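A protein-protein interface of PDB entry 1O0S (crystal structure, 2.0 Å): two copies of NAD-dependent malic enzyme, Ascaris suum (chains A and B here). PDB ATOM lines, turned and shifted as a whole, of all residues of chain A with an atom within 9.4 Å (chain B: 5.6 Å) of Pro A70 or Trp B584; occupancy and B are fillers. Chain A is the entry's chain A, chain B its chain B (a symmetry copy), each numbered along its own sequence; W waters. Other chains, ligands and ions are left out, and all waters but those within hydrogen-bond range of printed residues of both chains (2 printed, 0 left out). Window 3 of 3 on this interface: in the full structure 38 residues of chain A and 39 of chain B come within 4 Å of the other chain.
Printed residues of chain B that touch a printed residue of chain A: Tyr B582, Asp B583, Trp B584, Asp B588 and Met B589. Hydrophobic or aromatic side chains of chain B within 4 Å of the printed part of chain A: Tyr B582, Trp B584 and Met B589. Along chain B the printed residues that touch a printed residue of chain A span positions 582 to 589. Of the 17 printed residues of chain A, 6 touch a printed residue of chain B. Hydrophobic or aromatic side chains of chain A that line the printed part of chain B: Leu A56, Tyr A57, His A65, Pro A70 and Phe A72. Among the printed residues, no Asp or Glu carboxylate lies within 4 Å of a Lys or Arg side-chain nitrogen of the other chain.
The side-chain amide oxygen (OE1) of Gln A60 sits at hydrogen-bond distance from the backbone NH (N) of Tyr B582. OH of Tyr A57 lies close to OD1 of Asp B583, 2.4 Å away. A ring nitrogen (NE2) of His A65 sits close to the side-chain hydroxyl (OH) of Tyr B582 (3.4 Å).
The backbone NH (N) of His A65 lies within hydrogen-bond range of the backbone carbonyl oxygen (O) of Arg A59 (2.9 Å). SD of Met B589 lies within hydrogen-bond range of N of Trp B584, 3.4 Å away.
No position is printed for both chains. Of the 11 pairs that touch across the chains among the printed residues, none has its exchanged pair printed and touching as well.
Pro A70 touches one residue of chain B. Of chain A, only Leu A56 (3.7 Å), His A65 (3.5 Å), Pro A70 (3.7 Å) and Phe A72 (3.7 Å) come within 4 Å of Trp B584. Of the printed residues of chain B, Phe A72 touches Trp B584 (3.7 Å), Asp B588 (3.2 Å) and Met B589 (3.8 Å). Of the printed residues of chain B, Gln A60 touches Tyr B582. Of the printed residues of chain B, Leu A56 touches Tyr B582 (3.5 Å), Trp B584 (3.7 Å) and Met B589 (3.5 Å). Met A73 touches none of the printed residues of chain B. Leu A64 touches none of the printed residues of chain B. The nearest residue of chain A that does not touch Trp B584 is Gln A60 (5.0 Å). The nearest printed residue of chain B that does not touch Tyr A57 is Tyr B582 (4.2 Å).
Water W2 bridges O of Pro A70 (2.7 Å) and O of Asp B588 (2.8 Å). Water W1 lies within hydrogen-bond range of N of Leu A56 and O of Met B589.
Among the printed residues, pairs that only touch across the chains: Leu A56 with Tyr B582 (3.5 Å), Leu A56 with Trp B584 (3.7 Å), Leu A56 with Met B589 (3.5 Å), His A65 with Trp B584 (3.5 Å), Pro A70 with Trp B584 (3.7 Å), Phe A72 with Trp B584 (3.7 Å), Phe A72 with Asp B588 (3.2 Å) and Phe A72 with Met B589 (3.8 Å).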
ATOM      1  N   MET A  52      15.327  -4.140 -17.274  1.00  0.00           N
ATOM      2  CA  MET A  52      14.068  -4.021 -17.996  1.00  0.00           C
ATOM      3  C   MET A  52      14.254  -4.345 -19.468  1.00  0.00           C
ATOM      4  O   MET A  52      13.315  -4.246 -20.264  1.00  0.00           O
ATOM      5  CB  MET A  52      13.475  -2.621 -17.819  1.00  0.00           C
ATOM      6  CG  MET A  52      13.005  -2.358 -16.403  1.00  0.00           C
ATOM      7  SD  MET A  52      12.405  -0.684 -16.125  1.00  0.00           S
ATOM      8  CE  MET A  52      13.979   0.164 -15.982  1.00  0.00           C
ATOM      9  N   PHE A  54      14.788  -7.185 -20.378  1.00  0.00           N
ATOM     10  CA  PHE A  54      14.233  -8.537 -20.430  1.00  0.00           C
ATOM     11  C   PHE A  54      12.805  -8.456 -20.989  1.00  0.00           C
ATOM     12  O   PHE A  54      11.989  -7.664 -20.513  1.00  0.00           O
ATOM     13  CB  PHE A  54      14.163  -9.134 -19.016  1.00  0.00           C
ATOM     14  CG  PHE A  54      15.401  -9.876 -18.587  1.00  0.00           C
ATOM     15  CD1 PHE A  54      16.024  -9.566 -17.383  1.00  0.00           C
ATOM     16  CD2 PHE A  54      15.923 -10.908 -19.365  1.00  0.00           C
ATOM     17  CE1 PHE A  54      17.148 -10.275 -16.953  1.00  0.00           C
ATOM     18  CE2 PHE A  54      17.048 -11.624 -18.941  1.00  0.00           C
ATOM     19  CZ  PHE A  54      17.661 -11.301 -17.728  1.00  0.00           C
ATOM     20  N   SER A  55      12.489  -9.280 -21.980  1.00  0.00           N
ATOM     21  CA  SER A  55      11.145  -9.264 -22.543  1.00  0.00           C
ATOM     22  C   SER A  55      10.207  -9.950 -21.555  1.00  0.00           C
ATOM     23  O   SER A  55      10.662 -10.609 -20.627  1.00  0.00           O
ATOM     24  CB  SER A  55      11.107 -10.020 -23.871  1.00  0.00           C
ATOM     25  OG  SER A  55      11.276 -11.405 -23.650  1.00  0.00           O
ATOM     26  N   LEU A  56       8.904  -9.799 -21.776  1.00  0.00           N
ATOM     27  CA  LEU A  56       7.893 -10.405 -20.925  1.00  0.00           C
ATOM     28  C   LEU A  56       8.038 -11.929 -20.922  1.00  0.00           C
ATOM     29  O   LEU A  56       7.939 -12.566 -19.865  1.00  0.00           O
ATOM     30  CB  LEU A  56       6.496 -10.001 -21.414  1.00  0.00           C
ATOM     31  CG  LEU A  56       5.259 -10.590 -20.732  1.00  0.00           C
ATOM     32  CD1 LEU A  56       5.160 -10.129 -19.287  1.00  0.00           C
ATOM     33  CD2 LEU A  56       4.029 -10.159 -21.507  1.00  0.00           C
ATOM     34  N   TYR A  57       8.282 -12.523 -22.091  1.00  0.00           N
ATOM     35  CA  TYR A  57       8.425 -13.974 -22.154  1.00  0.00           C
ATOM     36  C   TYR A  57       9.655 -14.411 -21.383  1.00  0.00           C
ATOM     37  O   TYR A  57       9.620 -15.416 -20.671  1.00  0.00           O
ATOM     38  CB  TYR A  57       8.515 -14.477 -23.601  1.00  0.00           C
ATOM     39  CG  TYR A  57       7.269 -14.198 -24.419  1.00  0.00           C
ATOM     40  CD1 TYR A  57       5.998 -14.176 -23.821  1.00  0.00           C
ATOM     41  CD2 TYR A  57       7.354 -13.958 -25.792  1.00  0.00           C
ATOM     42  CE1 TYR A  57       4.852 -13.918 -24.575  1.00  0.00           C
ATOM     43  CE2 TYR A  57       6.215 -13.703 -26.554  1.00  0.00           C
ATOM     44  CZ  TYR A  57       4.971 -13.682 -25.944  1.00  0.00           C
ATOM     45  OH  TYR A  57       3.860 -13.423 -26.711  1.00  0.00           O
ATOM     46  N   ARG A  59      11.018 -12.907 -18.838  1.00  0.00           N
ATOM     47  CA  ARG A  59      10.764 -12.724 -17.417  1.00  0.00           C
ATOM     48  C   ARG A  59       9.920 -13.827 -16.826  1.00  0.00           C
ATOM     49  O   ARG A  59      10.119 -14.221 -15.682  1.00  0.00           O
ATOM     50  CB  ARG A  59      10.073 -11.384 -17.153  1.00  0.00           C
ATOM     51  CG  ARG A  59      10.919 -10.168 -17.509  1.00  0.00           C
ATOM     52  CD  ARG A  59      10.190  -8.877 -17.206  1.00  0.00           C
ATOM     53  NE  ARG A  59      10.849  -7.752 -17.864  1.00  0.00           N
ATOM     54  CZ  ARG A  59      10.556  -6.476 -17.644  1.00  0.00           C
ATOM     55  NH1 ARG A  59       9.610  -6.152 -16.774  1.00  0.00           N
ATOM     56  NH2 ARG A  59      11.215  -5.526 -18.296  1.00  0.00           N
ATOM     57  N   GLN A  60       8.963 -14.317 -17.600  1.00  0.00           N
ATOM     58  CA  GLN A  60       8.086 -15.379 -17.124  1.00  0.00           C
ATOM     59  C   GLN A  60       8.817 -16.724 -17.071  1.00  0.00           C
ATOM     60  O   GLN A  60       8.710 -17.465 -16.085  1.00  0.00           O
ATOM     61  CB  GLN A  60       6.851 -15.456 -18.021  1.00  0.00           C
ATOM     62  CG  GLN A  60       6.038 -14.159 -18.023  1.00  0.00           C
ATOM     63  CD  GLN A  60       4.925 -14.149 -19.052  1.00  0.00           C
ATOM     64  OE1 GLN A  60       4.991 -14.851 -20.057  1.00  0.00           O
ATOM     65  NE2 GLN A  60       3.902 -13.333 -18.813  1.00  0.00           N
ATOM     66  N   LEU A  64      11.576 -14.136 -13.384  1.00  0.00           N
ATOM     67  CA  LEU A  64      11.896 -12.736 -13.084  1.00  0.00           C
ATOM     68  C   LEU A  64      10.643 -11.847 -13.045  1.00  0.00           C
ATOM     69  O   LEU A  64      10.677 -10.724 -12.529  1.00  0.00           O
ATOM     70  CB  LEU A  64      12.818 -12.176 -14.165  1.00  0.00           C
ATOM     71  CG  LEU A  64      13.961 -13.045 -14.694  1.00  0.00           C
ATOM     72  CD1 LEU A  64      14.673 -12.325 -15.851  1.00  0.00           C
ATOM     73  CD2 LEU A  64      14.926 -13.331 -13.575  1.00  0.00           C
ATOM     74  N   HIS A  65       9.538 -12.345 -13.587  1.00  0.00           N
ATOM     75  CA  HIS A  65       8.337 -11.534 -13.665  1.00  0.00           C
ATOM     76  C   HIS A  65       7.830 -11.029 -12.323  1.00  0.00           C
ATOM     77  O   HIS A  65       7.645 -11.792 -11.377  1.00  0.00           O
ATOM     78  CB  HIS A  65       7.239 -12.277 -14.435  1.00  0.00           C
ATOM     79  CG  HIS A  65       6.124 -11.388 -14.894  1.00  0.00           C
ATOM     80  ND1 HIS A  65       6.350 -10.175 -15.518  1.00  0.00           N
ATOM     81  CD2 HIS A  65       4.776 -11.513 -14.796  1.00  0.00           C
ATOM     82  CE1 HIS A  65       5.191  -9.593 -15.776  1.00  0.00           C
ATOM     83  NE2 HIS A  65       4.219 -10.385 -15.346  1.00  0.00           N
ATOM     84  N   GLY A  66       7.616  -9.721 -12.247  1.00  0.00           N
ATOM     85  CA  GLY A  66       7.138  -9.125 -11.013  1.00  0.00           C
ATOM     86  C   GLY A  66       8.263  -8.525 -10.180  1.00  0.00           C
ATOM     87  O   GLY A  66       8.017  -7.649  -9.351  1.00  0.00           O
ATOM     88  N   LEU A  67       9.494  -8.982 -10.399  1.00  0.00           N
ATOM     89  CA  LEU A  67      10.641  -8.473  -9.652  1.00  0.00           C
ATOM     90  C   LEU A  67      11.205  -7.234 -10.337  1.00  0.00           C
ATOM     91  O   LEU A  67      12.062  -6.547  -9.784  1.00  0.00           O
ATOM     92  CB  LEU A  67      11.737  -9.541  -9.547  1.00  0.00           C
ATOM     93  CG  LEU A  67      11.496 -10.799  -8.709  1.00  0.00           C
ATOM     94  CD1 LEU A  67      12.553 -11.841  -9.036  1.00  0.00           C
ATOM     95  CD2 LEU A  67      11.560 -10.442  -7.218  1.00  0.00           C
ATOM     96  N   LEU A  68      10.732  -6.972 -11.550  1.00  0.00           N
ATOM     97  CA  LEU A  68      11.148  -5.804 -12.324  1.00  0.00           C
ATOM     98  C   LEU A  68       9.903  -4.957 -12.633  1.00  0.00           C
ATOM     99  O   LEU A  68       8.780  -5.468 -12.642  1.00  0.00           O
ATOM    100  CB  LEU A  68      11.792  -6.247 -13.639  1.00  0.00           C
ATOM    101  CG  LEU A  68      13.100  -7.038 -13.565  1.00  0.00           C
ATOM    102  CD1 LEU A  68      13.276  -7.864 -14.821  1.00  0.00           C
ATOM    103  CD2 LEU A  68      14.266  -6.083 -13.373  1.00  0.00           C
ATOM    104  N   PRO A  69      10.089  -3.647 -12.883  1.00  0.00           N
ATOM    105  CA  PRO A  69       8.989  -2.731 -13.201  1.00  0.00           C
ATOM    106  C   PRO A  69       8.337  -3.170 -14.524  1.00  0.00           C
ATOM    107  O   PRO A  69       9.000  -3.755 -15.388  1.00  0.00           O
ATOM    108  CB  PRO A  69       9.693  -1.372 -13.309  1.00  0.00           C
ATOM    109  CG  PRO A  69      10.840  -1.520 -12.374  1.00  0.00           C
ATOM    110  CD  PRO A  69      11.348  -2.904 -12.720  1.00  0.00           C
ATOM    111  N   PRO A  70       7.039  -2.877 -14.702  1.00  0.00           N
ATOM    112  CA  PRO A  70       6.311  -3.259 -15.916  1.00  0.00           C
ATOM    113  C   PRO A  70       6.623  -2.469 -17.179  1.00  0.00           C
ATOM    114  O   PRO A  70       5.732  -2.192 -17.979  1.00  0.00           O
ATOM    115  CB  PRO A  70       4.853  -3.115 -15.496  1.00  0.00           C
ATOM    116  CG  PRO A  70       4.898  -1.935 -14.596  1.00  0.00           C
ATOM    117  CD  PRO A  70       6.146  -2.180 -13.757  1.00  0.00           C
ATOM    118  N   ALA A  71       7.885  -2.104 -17.357  1.00  0.00           N
ATOM    119  CA  ALA A  71       8.297  -1.363 -18.536  1.00  0.00           C
ATOM    120  C   ALA A  71       9.318  -2.231 -19.237  1.00  0.00           C
ATOM    121  O   ALA A  71      10.107  -2.908 -18.579  1.00  0.00           O
ATOM    122  CB  ALA A  71       8.920  -0.019 -18.138  1.00  0.00           C
ATOM    123  N   PHE A  72       9.304  -2.217 -20.564  1.00  0.00           N
ATOM    124  CA  PHE A  72      10.236  -3.020 -21.348  1.00  0.00           C
ATOM    125  C   PHE A  72      11.097  -2.114 -22.212  1.00  0.00           C
ATOM    126  O   PHE A  72      10.595  -1.209 -22.868  1.00  0.00           O
ATOM    127  CB  PHE A  72       9.457  -4.015 -22.198  1.00  0.00           C
ATOM    128  CG  PHE A  72       8.512  -4.852 -21.397  1.00  0.00           C
ATOM    129  CD1 PHE A  72       7.257  -4.361 -21.045  1.00  0.00           C
ATOM    130  CD2 PHE A  72       8.909  -6.095 -20.906  1.00  0.00           C
ATOM    131  CE1 PHE A  72       6.400  -5.103 -20.213  1.00  0.00           C
ATOM    132  CE2 PHE A  72       8.065  -6.839 -20.078  1.00  0.00           C
ATOM    133  CZ  PHE A  72       6.810  -6.336 -19.728  1.00  0.00           C
ATOM    134  N   MET A  73      12.401  -2.355 -22.213  1.00  0.00           N
ATOM    135  CA  MET A  73      13.300  -1.501 -22.971  1.00  0.00           C
ATOM    136  C   MET A  73      14.245  -2.248 -23.888  1.00  0.00           C
ATOM    137  O   MET A  73      14.421  -3.461 -23.770  1.00  0.00           O
ATOM    138  CB  MET A  73      14.151  -0.669 -22.008  1.00  0.00           C
ATOM    139  CG  MET A  73      13.382   0.031 -20.907  1.00  0.00           C
ATOM    140  SD  MET A  73      14.487   0.926 -19.794  1.00  0.00           S
ATOM    141  CE  MET A  73      13.338   2.104 -19.019  1.00  0.00           C
ATOM    142  N   HIS B   5      -3.713 -12.686 -24.288  1.00  0.00           N
ATOM    143  CA  HIS B   5      -3.893 -11.741 -23.190  1.00  0.00           C
ATOM    144  C   HIS B   5      -5.223 -11.878 -22.452  1.00  0.00           C
ATOM    145  O   HIS B   5      -5.339 -11.466 -21.297  1.00  0.00           O
ATOM    146  CB  HIS B   5      -3.720 -10.303 -23.685  1.00  0.00           C
ATOM    147  CG  HIS B   5      -4.860  -9.806 -24.518  1.00  0.00           C
ATOM    148  ND1 HIS B   5      -6.129  -9.635 -24.014  1.00  0.00           N
ATOM    149  CD2 HIS B   5      -4.918  -9.445 -25.821  1.00  0.00           C
ATOM    150  CE1 HIS B   5      -6.925  -9.190 -24.971  1.00  0.00           C
ATOM    151  NE2 HIS B   5      -6.216  -9.066 -26.077  1.00  0.00           N
ATOM    152  N   TYR B 582       2.397 -15.974 -20.855  1.00  0.00           N
ATOM    153  CA  TYR B 582       1.155 -15.349 -21.285  1.00  0.00           C
ATOM    154  C   TYR B 582       1.360 -13.922 -21.775  1.00  0.00           C
ATOM    155  O   TYR B 582       2.257 -13.212 -21.312  1.00  0.00           O
ATOM    156  CB  TYR B 582       0.144 -15.382 -20.136  1.00  0.00           C
ATOM    157  CG  TYR B 582       0.559 -14.642 -18.885  1.00  0.00           C
ATOM    158  CD1 TYR B 582       0.191 -13.309 -18.687  1.00  0.00           C
ATOM    159  CD2 TYR B 582       1.304 -15.279 -17.888  1.00  0.00           C
ATOM    160  CE1 TYR B 582       0.554 -12.627 -17.523  1.00  0.00           C
ATOM    161  CE2 TYR B 582       1.674 -14.610 -16.724  1.00  0.00           C
ATOM    162  CZ  TYR B 582       1.297 -13.287 -16.546  1.00  0.00           C
ATOM    163  OH  TYR B 582       1.658 -12.630 -15.388  1.00  0.00           O
ATOM    164  N   ASP B 583       0.525 -13.516 -22.725  1.00  0.00           N
ATOM    165  CA  ASP B 583       0.595 -12.189 -23.310  1.00  0.00           C
ATOM    166  C   ASP B 583      -0.008 -11.119 -22.412  1.00  0.00           C
ATOM    167  O   ASP B 583      -0.791 -11.403 -21.512  1.00  0.00           O
ATOM    168  CB  ASP B 583      -0.163 -12.145 -24.642  1.00  0.00           C
ATOM    169  CG  ASP B 583       0.517 -12.921 -25.736  1.00  0.00           C
ATOM    170  OD1 ASP B 583       1.758 -12.854 -25.823  1.00  0.00           O
ATOM    171  OD2 ASP B 583      -0.194 -13.578 -26.527  1.00  0.00           O
ATOM    172  N   TRP B 584       0.374  -9.882 -22.699  1.00  0.00           N
ATOM    173  CA  TRP B 584      -0.126  -8.694 -22.023  1.00  0.00           C
ATOM    174  C   TRP B 584      -0.695  -7.898 -23.195  1.00  0.00           C
ATOM    175  O   TRP B 584      -0.448  -8.249 -24.348  1.00  0.00           O
ATOM    176  CB  TRP B 584       1.029  -7.893 -21.418  1.00  0.00           C
ATOM    177  CG  TRP B 584       1.288  -8.135 -19.970  1.00  0.00           C
ATOM    178  CD1 TRP B 584       0.876  -9.201 -19.223  1.00  0.00           C
ATOM    179  CD2 TRP B 584       2.052  -7.300 -19.095  1.00  0.00           C
ATOM    180  NE1 TRP B 584       1.336  -9.083 -17.931  1.00  0.00           N
ATOM    181  CE2 TRP B 584       2.061  -7.925 -17.824  1.00  0.00           C
ATOM    182  CE3 TRP B 584       2.734  -6.086 -19.261  1.00  0.00           C
ATOM    183  CZ2 TRP B 584       2.726  -7.367 -16.716  1.00  0.00           C
ATOM    184  CZ3 TRP B 584       3.397  -5.530 -18.156  1.00  0.00           C
ATOM    185  CH2 TRP B 584       3.386  -6.177 -16.903  1.00  0.00           C
ATOM    186  N   PRO B 585      -1.473  -6.836 -22.929  1.00  0.00           N
ATOM    187  CA  PRO B 585      -1.979  -6.096 -24.090  1.00  0.00           C
ATOM    188  C   PRO B 585      -0.766  -5.752 -24.960  1.00  0.00           C
ATOM    189  O   PRO B 585       0.300  -5.437 -24.439  1.00  0.00           O
ATOM    190  CB  PRO B 585      -2.611  -4.863 -23.460  1.00  0.00           C
ATOM    191  CG  PRO B 585      -3.153  -5.408 -22.162  1.00  0.00           C
ATOM    192  CD  PRO B 585      -2.032  -6.309 -21.671  1.00  0.00           C
ATOM    193  N   GLU B 586      -0.922  -5.829 -26.275  1.00  0.00           N
ATOM    194  CA  GLU B 586       0.180  -5.539 -27.185  1.00  0.00           C
ATOM    195  C   GLU B 586       0.910  -4.239 -26.857  1.00  0.00           C
ATOM    196  O   GLU B 586       2.128  -4.225 -26.652  1.00  0.00           O
ATOM    197  CB  GLU B 586      -0.339  -5.487 -28.619  1.00  0.00           C
ATOM    198  CG  GLU B 586       0.730  -5.186 -29.650  1.00  0.00           C
ATOM    199  CD  GLU B 586       0.185  -5.238 -31.059  1.00  0.00           C
ATOM    200  OE1 GLU B 586      -0.793  -4.511 -31.343  1.00  0.00           O
ATOM    201  OE2 GLU B 586       0.731  -6.009 -31.881  1.00  0.00           O
ATOM    202  N   ASP B 588       1.400  -2.748 -24.342  1.00  0.00           N
ATOM    203  CA  ASP B 588       2.191  -2.797 -23.111  1.00  0.00           C
ATOM    204  C   ASP B 588       3.370  -3.769 -23.016  1.00  0.00           C
ATOM    205  O   ASP B 588       3.957  -3.912 -21.942  1.00  0.00           O
ATOM    206  CB  ASP B 588       1.269  -3.030 -21.904  1.00  0.00           C
ATOM    207  CG  ASP B 588       0.255  -1.905 -21.703  1.00  0.00           C
ATOM    208  OD1 ASP B 588       0.621  -0.719 -21.864  1.00  0.00           O
ATOM    209  OD2 ASP B 588      -0.909  -2.204 -21.362  1.00  0.00           O
ATOM    210  N   MET B 589       3.724  -4.435 -24.111  1.00  0.00           N
ATOM    211  CA  MET B 589       4.860  -5.358 -24.080  1.00  0.00           C
ATOM    212  C   MET B 589       5.986  -4.803 -24.946  1.00  0.00           C
ATOM    213  O   MET B 589       7.101  -5.318 -24.934  1.00  0.00           O
ATOM    214  CB  MET B 589       4.480  -6.735 -24.629  1.00  0.00           C
ATOM    215  CG  MET B 589       3.238  -7.363 -24.045  1.00  0.00           C
ATOM    216  SD  MET B 589       3.049  -9.056 -24.675  1.00  0.00           S
ATOM    217  CE  MET B 589       3.039  -8.761 -26.458  1.00  0.00           C
HETATM  218  O   HOH W   1       8.257  -8.238 -24.122  1.00  0.00           O
HETATM  219  O   HOH W   2       4.406  -1.629 -20.298  1.00  0.00           O
